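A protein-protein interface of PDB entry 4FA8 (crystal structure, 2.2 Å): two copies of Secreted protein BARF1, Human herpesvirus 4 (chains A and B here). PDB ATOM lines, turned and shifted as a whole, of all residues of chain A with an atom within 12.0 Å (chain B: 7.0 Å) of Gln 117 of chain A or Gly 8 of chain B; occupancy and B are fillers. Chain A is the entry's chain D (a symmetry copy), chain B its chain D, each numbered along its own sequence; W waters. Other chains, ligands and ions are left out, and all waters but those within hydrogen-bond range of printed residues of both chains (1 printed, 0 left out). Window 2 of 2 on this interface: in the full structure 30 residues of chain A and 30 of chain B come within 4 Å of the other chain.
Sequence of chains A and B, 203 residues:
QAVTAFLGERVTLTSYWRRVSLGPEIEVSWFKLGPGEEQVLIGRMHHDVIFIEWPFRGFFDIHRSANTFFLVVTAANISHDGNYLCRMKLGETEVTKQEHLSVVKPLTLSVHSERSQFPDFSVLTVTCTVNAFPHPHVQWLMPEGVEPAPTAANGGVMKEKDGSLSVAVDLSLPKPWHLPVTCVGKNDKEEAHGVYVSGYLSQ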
ATOM      1  N   HIS A 112      23.308  12.209   7.970  1.00  0.00           N
ATOM      2  CA  HIS A 112      22.077  11.911   8.680  1.00  0.00           C
ATOM      3  C   HIS A 112      21.885  12.969   9.710  1.00  0.00           C
ATOM      4  O   HIS A 112      22.846  13.634  10.112  1.00  0.00           O
ATOM      5  CB  HIS A 112      22.145  10.542   9.332  1.00  0.00           C
ATOM      6  CG  HIS A 112      23.251  10.404  10.348  1.00  0.00           C
ATOM      7  ND1 HIS A 112      23.010  10.283  11.669  1.00  0.00           N
ATOM      8  CD2 HIS A 112      24.637  10.372  10.197  1.00  0.00           C
ATOM      9  CE1 HIS A 112      24.180  10.179  12.331  1.00  0.00           C
ATOM     10  NE2 HIS A 112      25.174  10.234  11.428  1.00  0.00           N
ATOM     11  N   SER A 113      20.643  13.157  10.140  1.00  0.00           N
ATOM     12  CA  SER A 113      20.353  14.170  11.142  1.00  0.00           C
ATOM     13  C   SER A 113      19.841  13.550  12.429  1.00  0.00           C
ATOM     14  O   SER A 113      19.517  12.361  12.482  1.00  0.00           O
ATOM     15  CB  SER A 113      19.350  15.195  10.606  1.00  0.00           C
ATOM     16  OG  SER A 113      18.055  14.636  10.444  1.00  0.00           O
ATOM     17  N   GLU A 114      19.791  14.372  13.470  1.00  0.00           N
ATOM     18  CA  GLU A 114      19.219  13.990  14.747  1.00  0.00           C
ATOM     19  C   GLU A 114      18.729  15.243  15.454  1.00  0.00           C
ATOM     20  O   GLU A 114      19.495  16.195  15.626  1.00  0.00           O
ATOM     21  CB  GLU A 114      20.263  13.270  15.596  1.00  0.00           C
ATOM     22  CG  GLU A 114      19.722  12.672  16.881  1.00  0.00           C
ATOM     23  CD  GLU A 114      20.785  11.966  17.686  1.00  0.00           C
ATOM     24  OE1 GLU A 114      21.676  11.331  17.088  1.00  0.00           O
ATOM     25  OE2 GLU A 114      20.733  12.042  18.925  1.00  0.00           O
ATOM     26  N   ARG A 115      17.458  15.261  15.852  1.00  0.00           N
ATOM     27  CA  ARG A 115      16.968  16.364  16.673  1.00  0.00           C
ATOM     28  C   ARG A 115      17.312  16.135  18.146  1.00  0.00           C
ATOM     29  O   ARG A 115      17.480  14.991  18.583  1.00  0.00           O
ATOM     30  CB  ARG A 115      15.470  16.618  16.461  1.00  0.00           C
ATOM     31  CG  ARG A 115      14.536  15.700  17.229  1.00  0.00           C
ATOM     32  CD  ARG A 115      13.091  16.049  16.937  1.00  0.00           C
ATOM     33  NE  ARG A 115      12.174  15.121  17.592  1.00  0.00           N
ATOM     34  CZ  ARG A 115      10.858  15.293  17.705  1.00  0.00           C
ATOM     35  NH1 ARG A 115      10.268  16.366  17.211  1.00  0.00           N
ATOM     36  NH2 ARG A 115      10.134  14.381  18.326  1.00  0.00           N
ATOM     37  N   SER A 116      17.435  17.227  18.897  1.00  0.00           N
ATOM     38  CA  SER A 116      17.730  17.153  20.318  1.00  0.00           C
ATOM     39  C   SER A 116      16.544  16.613  21.112  1.00  0.00           C
ATOM     40  O   SER A 116      15.402  16.657  20.650  1.00  0.00           O
ATOM     41  CB  SER A 116      18.141  18.525  20.855  1.00  0.00           C
ATOM     42  OG  SER A 116      17.159  19.499  20.554  1.00  0.00           O
ATOM     43  N   GLN A 117      16.829  16.105  22.308  1.00  0.00           N
ATOM     44  CA  GLN A 117      15.810  15.553  23.184  1.00  0.00           C
ATOM     45  C   GLN A 117      15.730  16.322  24.493  1.00  0.00           C
ATOM     46  O   GLN A 117      14.794  16.135  25.254  1.00  0.00           O
ATOM     47  CB  GLN A 117      16.100  14.084  23.476  1.00  0.00           C
ATOM     48  CG  GLN A 117      16.008  13.171  22.272  1.00  0.00           C
ATOM     49  CD  GLN A 117      16.651  11.819  22.516  1.00  0.00           C
ATOM     50  OE1 GLN A 117      16.405  11.157  23.535  1.00  0.00           O
ATOM     51  NE2 GLN A 117      17.478  11.395  21.576  1.00  0.00           N
ATOM     52  N   PHE A 118      16.727  17.165  24.753  1.00  0.00           N
ATOM     53  CA  PHE A 118      16.745  18.029  25.932  1.00  0.00           C
ATOM     54  C   PHE A 118      17.531  19.327  25.666  1.00  0.00           C
ATOM     55  O   PHE A 118      18.559  19.292  24.985  1.00  0.00           O
ATOM     56  CB  PHE A 118      17.295  17.292  27.159  1.00  0.00           C
ATOM     57  CG  PHE A 118      16.876  17.909  28.467  1.00  0.00           C
ATOM     58  CD1 PHE A 118      17.716  18.787  29.140  1.00  0.00           C
ATOM     59  CD2 PHE A 118      15.622  17.640  29.009  1.00  0.00           C
ATOM     60  CE1 PHE A 118      17.326  19.375  30.332  1.00  0.00           C
ATOM     61  CE2 PHE A 118      15.222  18.227  30.199  1.00  0.00           C
ATOM     62  CZ  PHE A 118      16.078  19.091  30.864  1.00  0.00           C
ATOM     63  N   PRO A 119      17.038  20.484  26.181  1.00  0.00           N
ATOM     64  CA  PRO A 119      15.784  20.637  26.941  1.00  0.00           C
ATOM     65  C   PRO A 119      14.523  20.583  26.073  1.00  0.00           C
ATOM     66  O   PRO A 119      13.423  20.491  26.602  1.00  0.00           O
ATOM     67  CB  PRO A 119      15.937  21.997  27.614  1.00  0.00           C
ATOM     68  CG  PRO A 119      16.847  22.753  26.717  1.00  0.00           C
ATOM     69  CD  PRO A 119      17.777  21.757  26.086  1.00  0.00           C
ATOM     70  N   ASP A 120      14.684  20.631  24.756  1.00  0.00           N
ATOM     71  CA  ASP A 120      13.559  20.460  23.839  1.00  0.00           C
ATOM     72  C   ASP A 120      14.017  19.840  22.526  1.00  0.00           C
ATOM     73  O   ASP A 120      15.171  19.452  22.390  1.00  0.00           O
ATOM     74  CB  ASP A 120      12.823  21.789  23.598  1.00  0.00           C
ATOM     75  CG  ASP A 120      13.683  22.825  22.896  1.00  0.00           C
ATOM     76  OD1 ASP A 120      13.485  24.019  23.171  1.00  0.00           O
ATOM     77  OD2 ASP A 120      14.549  22.465  22.069  1.00  0.00           O
ATOM     78  N   PHE A 121      13.112  19.791  21.555  1.00  0.00           N
ATOM     79  CA  PHE A 121      13.347  19.110  20.291  1.00  0.00           C
ATOM     80  C   PHE A 121      13.634  20.079  19.149  1.00  0.00           C
ATOM     81  O   PHE A 121      13.477  19.727  17.976  1.00  0.00           O
ATOM     82  CB  PHE A 121      12.126  18.254  19.952  1.00  0.00           C
ATOM     83  CG  PHE A 121      11.698  17.343  21.066  1.00  0.00           C
ATOM     84  CD1 PHE A 121      10.764  17.758  22.002  1.00  0.00           C
ATOM     85  CD2 PHE A 121      12.227  16.064  21.177  1.00  0.00           C
ATOM     86  CE1 PHE A 121      10.371  16.917  23.033  1.00  0.00           C
ATOM     87  CE2 PHE A 121      11.840  15.217  22.204  1.00  0.00           C
ATOM     88  CZ  PHE A 121      10.909  15.644  23.131  1.00  0.00           C
ATOM     89  N   SER A 122      14.059  21.296  19.485  1.00  0.00           N
ATOM     90  CA  SER A 122      14.187  22.367  18.491  1.00  0.00           C
ATOM     91  C   SER A 122      15.550  22.456  17.793  1.00  0.00           C
ATOM     92  O   SER A 122      15.696  23.164  16.801  1.00  0.00           O
ATOM     93  CB  SER A 122      13.837  23.712  19.119  1.00  0.00           C
ATOM     94  OG  SER A 122      14.818  24.079  20.067  1.00  0.00           O
ATOM     95  N   VAL A 123      16.545  21.743  18.309  1.00  0.00           N
ATOM     96  CA  VAL A 123      17.879  21.782  17.718  1.00  0.00           C
ATOM     97  C   VAL A 123      18.081  20.580  16.806  1.00  0.00           C
ATOM     98  O   VAL A 123      17.887  19.440  17.217  1.00  0.00           O
ATOM     99  CB  VAL A 123      18.995  21.830  18.787  1.00  0.00           C
ATOM    100  CG1 VAL A 123      20.369  21.779  18.136  1.00  0.00           C
ATOM    101  CG2 VAL A 123      18.861  23.080  19.630  1.00  0.00           C
ATOM    102  N   LEU A 124      18.458  20.845  15.562  1.00  0.00           N
ATOM    103  CA  LEU A 124      18.842  19.794  14.642  1.00  0.00           C
ATOM    104  C   LEU A 124      20.360  19.791  14.524  1.00  0.00           C
ATOM    105  O   LEU A 124      20.959  20.796  14.136  1.00  0.00           O
ATOM    106  CB  LEU A 124      18.192  20.014  13.271  1.00  0.00           C
ATOM    107  CG  LEU A 124      18.283  18.911  12.207  1.00  0.00           C
ATOM    108  CD1 LEU A 124      17.500  17.678  12.617  1.00  0.00           C
ATOM    109  CD2 LEU A 124      17.783  19.417  10.861  1.00  0.00           C
ATOM    110  N   THR A 125      20.987  18.680  14.902  1.00  0.00           N
ATOM    111  CA  THR A 125      22.388  18.477  14.552  1.00  0.00           C
ATOM    112  C   THR A 125      22.538  17.463  13.422  1.00  0.00           C
ATOM    113  O   THR A 125      22.059  16.335  13.497  1.00  0.00           O
ATOM    114  CB  THR A 125      23.335  18.188  15.748  1.00  0.00           C
ATOM    115  OG1 THR A 125      24.224  17.116  15.409  1.00  0.00           O
ATOM    116  CG2 THR A 125      22.588  17.836  16.980  1.00  0.00           C
ATOM    117  N   VAL A 126      23.178  17.911  12.354  1.00  0.00           N
ATOM    118  CA  VAL A 126      23.362  17.085  11.185  1.00  0.00           C
ATOM    119  C   VAL A 126      24.835  16.661  11.123  1.00  0.00           C
ATOM    120  O   VAL A 126      25.742  17.454  11.418  1.00  0.00           O
ATOM    121  CB  VAL A 126      22.779  17.768   9.912  1.00  0.00           C
ATOM    122  CG1 VAL A 126      23.431  19.113   9.647  1.00  0.00           C
ATOM    123  CG2 VAL A 126      22.856  16.858   8.693  1.00  0.00           C
ATOM    124  N   SER A 172      25.147  22.088  14.282  1.00  0.00           N
ATOM    125  CA  SER A 172      23.926  22.254  15.067  1.00  0.00           C
ATOM    126  C   SER A 172      23.117  23.483  14.661  1.00  0.00           C
ATOM    127  O   SER A 172      23.603  24.612  14.712  1.00  0.00           O
ATOM    128  CB  SER A 172      24.248  22.287  16.560  1.00  0.00           C
ATOM    129  OG  SER A 172      24.699  21.013  16.984  1.00  0.00           O
ATOM    130  N   LEU A 173      21.871  23.245  14.268  1.00  0.00           N
ATOM    131  CA  LEU A 173      20.993  24.298  13.798  1.00  0.00           C
ATOM    132  C   LEU A 173      19.876  24.523  14.805  1.00  0.00           C
ATOM    133  O   LEU A 173      19.133  23.592  15.119  1.00  0.00           O
ATOM    134  CB  LEU A 173      20.395  23.917  12.442  1.00  0.00           C
ATOM    135  CG  LEU A 173      21.323  23.496  11.293  1.00  0.00           C
ATOM    136  CD1 LEU A 173      20.515  22.892  10.150  1.00  0.00           C
ATOM    137  CD2 LEU A 173      22.156  24.668  10.795  1.00  0.00           C
ATOM    138  N   PRO A 174      19.767  25.752  15.340  1.00  0.00           N
ATOM    139  CA  PRO A 174      18.607  26.105  16.156  1.00  0.00           C
ATOM    140  C   PRO A 174      17.438  26.490  15.263  1.00  0.00           C
ATOM    141  O   PRO A 174      17.635  26.724  14.071  1.00  0.00           O
ATOM    142  CB  PRO A 174      19.090  27.325  16.954  1.00  0.00           C
ATOM    143  CG  PRO A 174      20.566  27.408  16.731  1.00  0.00           C
ATOM    144  CD  PRO A 174      20.801  26.798  15.390  1.00  0.00           C
ATOM    145  N   LYS A 175      16.237  26.541  15.829  1.00  0.00           N
ATOM    146  CA  LYS A 175      15.048  26.975  15.089  1.00  0.00           C
ATOM    147  C   LYS A 175      15.075  28.475  14.775  1.00  0.00           C
ATOM    148  O   LYS A 175      15.545  29.270  15.590  1.00  0.00           O
ATOM    149  CB  LYS A 175      13.769  26.640  15.854  1.00  0.00           C
ATOM    150  CG  LYS A 175      13.386  25.166  15.853  1.00  0.00           C
ATOM    151  CD  LYS A 175      12.836  24.692  14.516  1.00  0.00           C
ATOM    152  CE  LYS A 175      12.079  23.378  14.675  1.00  0.00           C
ATOM    153  NZ  LYS A 175      11.737  22.781  13.352  1.00  0.00           N
ATOM    154  N   TRP A 177      15.420  26.246  11.257  1.00  0.00           N
ATOM    155  CA  TRP A 177      16.584  25.614  10.639  1.00  0.00           C
ATOM    156  C   TRP A 177      16.877  26.179   9.283  1.00  0.00           C
ATOM    157  O   TRP A 177      15.999  26.224   8.421  1.00  0.00           O
ATOM    158  CB  TRP A 177      16.373  24.107  10.532  1.00  0.00           C
ATOM    159  CG  TRP A 177      16.056  23.418  11.838  1.00  0.00           C
ATOM    160  CD1 TRP A 177      16.478  23.777  13.119  1.00  0.00           C
ATOM    161  CD2 TRP A 177      15.262  22.194  12.029  1.00  0.00           C
ATOM    162  NE1 TRP A 177      16.000  22.898  14.055  1.00  0.00           N
ATOM    163  CE2 TRP A 177      15.265  21.924  13.470  1.00  0.00           C
ATOM    164  CE3 TRP A 177      14.575  21.328  11.182  1.00  0.00           C
ATOM    165  CZ2 TRP A 177      14.607  20.827  14.015  1.00  0.00           C
ATOM    166  CZ3 TRP A 177      13.911  20.230  11.744  1.00  0.00           C
ATOM    167  CH2 TRP A 177      13.926  19.990  13.126  1.00  0.00           C
ATOM    168  N   ALA B   5       7.446   9.898  16.998  1.00  0.00           N
ATOM    169  CA  ALA B   5       8.648   9.829  17.814  1.00  0.00           C
ATOM    170  C   ALA B   5       9.815   9.426  16.933  1.00  0.00           C
ATOM    171  O   ALA B   5       9.650   8.662  15.986  1.00  0.00           O
ATOM    172  CB  ALA B   5       8.463   8.810  18.922  1.00  0.00           C
ATOM    173  N   PHE B   6      11.001   9.932  17.230  1.00  0.00           N
ATOM    174  CA  PHE B   6      12.163   9.435  16.522  1.00  0.00           C
ATOM    175  C   PHE B   6      12.793   8.285  17.286  1.00  0.00           C
ATOM    176  O   PHE B   6      12.551   8.116  18.480  1.00  0.00           O
ATOM    177  CB  PHE B   6      13.149  10.557  16.214  1.00  0.00           C
ATOM    178  CG  PHE B   6      12.634  11.542  15.206  1.00  0.00           C
ATOM    179  CD1 PHE B   6      11.997  12.705  15.617  1.00  0.00           C
ATOM    180  CD2 PHE B   6      12.757  11.292  13.843  1.00  0.00           C
ATOM    181  CE1 PHE B   6      11.513  13.616  14.690  1.00  0.00           C
ATOM    182  CE2 PHE B   6      12.274  12.196  12.911  1.00  0.00           C
ATOM    183  CZ  PHE B   6      11.651  13.362  13.335  1.00  0.00           C
ATOM    184  N   LEU B   7      13.558   7.470  16.568  1.00  0.00           N
ATOM    185  CA  LEU B   7      14.232   6.322  17.133  1.00  0.00           C
ATOM    186  C   LEU B   7      15.066   6.755  18.327  1.00  0.00           C
ATOM    187  O   LEU B   7      15.842   7.703  18.233  1.00  0.00           O
ATOM    188  CB  LEU B   7      15.121   5.672  16.063  1.00  0.00           C
ATOM    189  CG  LEU B   7      15.494   4.201  16.231  1.00  0.00           C
ATOM    190  CD1 LEU B   7      14.287   3.316  15.935  1.00  0.00           C
ATOM    191  CD2 LEU B   7      16.644   3.842  15.306  1.00  0.00           C
ATOM    192  N   GLY B   8      14.869   6.093  19.460  1.00  0.00           N
ATOM    193  CA  GLY B   8      15.615   6.426  20.664  1.00  0.00           C
ATOM    194  C   GLY B   8      14.924   7.412  21.585  1.00  0.00           C
ATOM    195  O   GLY B   8      15.300   7.535  22.750  1.00  0.00           O
ATOM    196  N   GLU B   9      13.911   8.111  21.081  1.00  0.00           N
ATOM    197  CA  GLU B   9      13.210   9.112  21.894  1.00  0.00           C
ATOM    198  C   GLU B   9      12.249   8.522  22.915  1.00  0.00           C
ATOM    199  O   GLU B   9      11.590   7.503  22.665  1.00  0.00           O
ATOM    200  CB  GLU B   9      12.470  10.122  21.022  1.00  0.00           C
ATOM    201  CG  GLU B   9      13.390  11.077  20.288  1.00  0.00           C
ATOM    202  CD  GLU B   9      12.645  12.065  19.414  1.00  0.00           C
ATOM    203  OE1 GLU B   9      11.426  11.895  19.226  1.00  0.00           O
ATOM    204  OE2 GLU B   9      13.282  13.010  18.904  1.00  0.00           O
ATOM    205  N   ARG B  10      12.188   9.174  24.073  1.00  0.00           N
ATOM    206  CA  ARG B  10      11.127   8.943  25.034  1.00  0.00           C
ATOM    207  C   ARG B  10       9.874   9.595  24.470  1.00  0.00           C
ATOM    208  O   ARG B  10       9.914  10.724  24.002  1.00  0.00           O
ATOM    209  CB  ARG B  10      11.471   9.590  26.359  1.00  0.00           C
ATOM    210  CG  ARG B  10      10.455   9.302  27.446  1.00  0.00           C
ATOM    211  CD  ARG B  10      10.701  10.190  28.637  1.00  0.00           C
ATOM    212  NE  ARG B  10       9.823   9.878  29.759  1.00  0.00           N
ATOM    213  CZ  ARG B  10       8.691  10.520  30.024  1.00  0.00           C
ATOM    214  NH1 ARG B  10       8.282  11.505  29.242  1.00  0.00           N
ATOM    215  NH2 ARG B  10       7.974  10.170  31.077  1.00  0.00           N
ATOM    216  N   VAL B  11       8.765   8.882  24.488  1.00  0.00           N
ATOM    217  CA  VAL B  11       7.535   9.452  23.962  1.00  0.00           C
ATOM    218  C   VAL B  11       6.384   8.974  24.818  1.00  0.00           C
ATOM    219  O   VAL B  11       6.533   8.021  25.578  1.00  0.00           O
ATOM    220  CB  VAL B  11       7.350   9.148  22.453  1.00  0.00           C
ATOM    221  CG1 VAL B  11       7.196   7.655  22.209  1.00  0.00           C
ATOM    222  CG2 VAL B  11       6.204   9.957  21.848  1.00  0.00           C
ATOM    223  N   VAL B  73       6.765   5.091  26.496  1.00  0.00           N
ATOM    224  CA  VAL B  73       7.711   4.216  25.847  1.00  0.00           C
ATOM    225  C   VAL B  73       9.055   4.901  25.986  1.00  0.00           C
ATOM    226  O   VAL B  73       9.280   5.978  25.436  1.00  0.00           O
ATOM    227  CB  VAL B  73       7.326   3.894  24.387  1.00  0.00           C
ATOM    228  CG1 VAL B  73       6.414   4.958  23.829  1.00  0.00           C
ATOM    229  CG2 VAL B  73       8.553   3.671  23.507  1.00  0.00           C
ATOM    230  N   THR B  74       9.931   4.251  26.742  1.00  0.00           N
ATOM    231  CA  THR B  74      11.163   4.855  27.237  1.00  0.00           C
ATOM    232  C   THR B  74      12.227   5.171  26.177  1.00  0.00           C
ATOM    233  O   THR B  74      12.983   6.126  26.336  1.00  0.00           O
ATOM    234  CB  THR B  74      11.754   4.022  28.388  1.00  0.00           C
ATOM    235  OG1 THR B  74      11.853   2.652  27.990  1.00  0.00           O
ATOM    236  CG2 THR B  74      10.862   4.112  29.625  1.00  0.00           C
ATOM    237  N   ALA B  75      12.286   4.367  25.114  1.00  0.00           N
ATOM    238  CA  ALA B  75      13.216   4.580  23.993  1.00  0.00           C
ATOM    239  C   ALA B  75      12.618   4.026  22.713  1.00  0.00           C
ATOM    240  O   ALA B  75      12.760   2.838  22.417  1.00  0.00           O
ATOM    241  CB  ALA B  75      14.548   3.909  24.267  1.00  0.00           C
ATOM    242  N   ALA B  76      11.963   4.883  21.940  1.00  0.00           N
ATOM    243  CA  ALA B  76      11.182   4.401  20.797  1.00  0.00           C
ATOM    244  C   ALA B  76      12.049   3.572  19.861  1.00  0.00           C
ATOM    245  O   ALA B  76      13.119   4.014  19.427  1.00  0.00           O
ATOM    246  CB  ALA B  76      10.532   5.555  20.048  1.00  0.00           C
ATOM    247  N   ASN B  77      11.668   2.270  19.605  1.00  0.00           N
ATOM    248  CA  ASN B  77      12.302   1.482  18.561  1.00  0.00           C
ATOM    249  C   ASN B  77      11.251   1.108  17.536  1.00  0.00           C
ATOM    250  O   ASN B  77      10.055   1.307  17.774  1.00  0.00           O
ATOM    251  CB  ASN B  77      13.060   0.270  19.126  1.00  0.00           C
ATOM    252  CG  ASN B  77      12.158  -0.907  19.504  1.00  0.00           C
ATOM    253  OD1 ASN B  77      11.055  -1.084  18.982  1.00  0.00           O
ATOM    254  ND2 ASN B  77      12.668  -1.742  20.413  1.00  0.00           N
ATOM    255  N   VAL B 103       6.939   5.718  14.662  1.00  0.00           N
ATOM    256  CA  VAL B 103       8.368   5.746  14.929  1.00  0.00           C
ATOM    257  C   VAL B 103       9.073   6.023  13.617  1.00  0.00           C
ATOM    258  O   VAL B 103       8.717   5.476  12.570  1.00  0.00           O
ATOM    259  CB  VAL B 103       8.907   4.453  15.557  1.00  0.00           C
ATOM    260  CG1 VAL B 103      10.346   4.662  16.006  1.00  0.00           C
ATOM    261  CG2 VAL B 103       8.055   4.040  16.747  1.00  0.00           C
ATOM    262  N   VAL B 104      10.059   6.906  13.678  1.00  0.00           N
ATOM    263  CA  VAL B 104      10.766   7.344  12.493  1.00  0.00           C
ATOM    264  C   VAL B 104      12.266   7.236  12.736  1.00  0.00           C
ATOM    265  O   VAL B 104      12.771   7.655  13.790  1.00  0.00           O
ATOM    266  CB  VAL B 104      10.351   8.784  12.121  1.00  0.00           C
ATOM    267  CG1 VAL B 104      11.249   9.356  11.023  1.00  0.00           C
ATOM    268  CG2 VAL B 104       8.883   8.810  11.699  1.00  0.00           C
HETATM  269  O   HOH W   1      14.051  11.070  25.094  1.00  0.00           O
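The guanidinium group (NE) of Arg 115 of chain A lies within salt-bridge range of the side-chain carboxylate (OE2) of Glu 9 of chain B (2.7 Å).
The backbone NH (N) of Phe 6 of chain B lies within hydrogen-bond range of the side-chain carboxylate (OE1) of Glu 9 of chain B. O of Ala 76 of chain B is in hydrogen-bond range of N of Gly 8 of chain B, at 2.7 Å. N of Ala 76 of chain B is in hydrogen-bond range of O of Glu 9 of chain B, 2.7 Å away.
Among the printed residues, pairs that only touch across the chains: Arg 115 of chain A with Phe 6 of chain B, Gln 117 of chain A with Gly 8 of chain B, Gln 117 of chain A with Glu 9 of chain B and Phe 121 of chain A with Glu 9 of chain B.
Printed residues of chain B within 4 Å of Arg 115 of chain A: Phe 6 and Glu 9. Gln 117 of chain A touches two residues of chain B. Of the printed residues of chain B, Phe 121 of chain A touches Glu 9. Ser 172 of chain A touches none of the printed residues of chain B. Of the printed residues of chain A, Phe 6 of chain B touches Arg 115 (3.1 Å). No residue of chain A comes within 4 Å of Leu 7 of chain B. Gly 8 of chain B touches just one residue of chain A: Gln 117 (3.9 Å). Glu 9 of chain B touches just these residues of chain A: Arg 115 (2.7 Å), Gln 117 (3.9 Å) and Phe 121 (3.95 Å). The nearest residue of chain A that does not touch Gly 8 of chain B is Glu 114 of chain A (7.8 Å). The nearest printed residue of chain B that does not touch Phe 121 of chain A is Arg 10 of chain B (5.1 Å).
Hydrophobic or aromatic side chains of chain A that line the printed part of chain B: Phe 121. Among the printed residues, Asp or Glu carboxylates within 4 Å of a Lys or Arg side-chain nitrogen of the other chain: Arg 115 of chain A with Glu 9 of chain B (2.7 Å).
No position is printed for both chains. Of the 5 pairs that touch across the chains among the printed residues, none has its exchanged pair printed and touching as well.
Water W1 lies within hydrogen-bond range of OE1 of Gln 117 of chain A (2.8 Å) and N of Arg 10 of chain B (2.8 Å).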
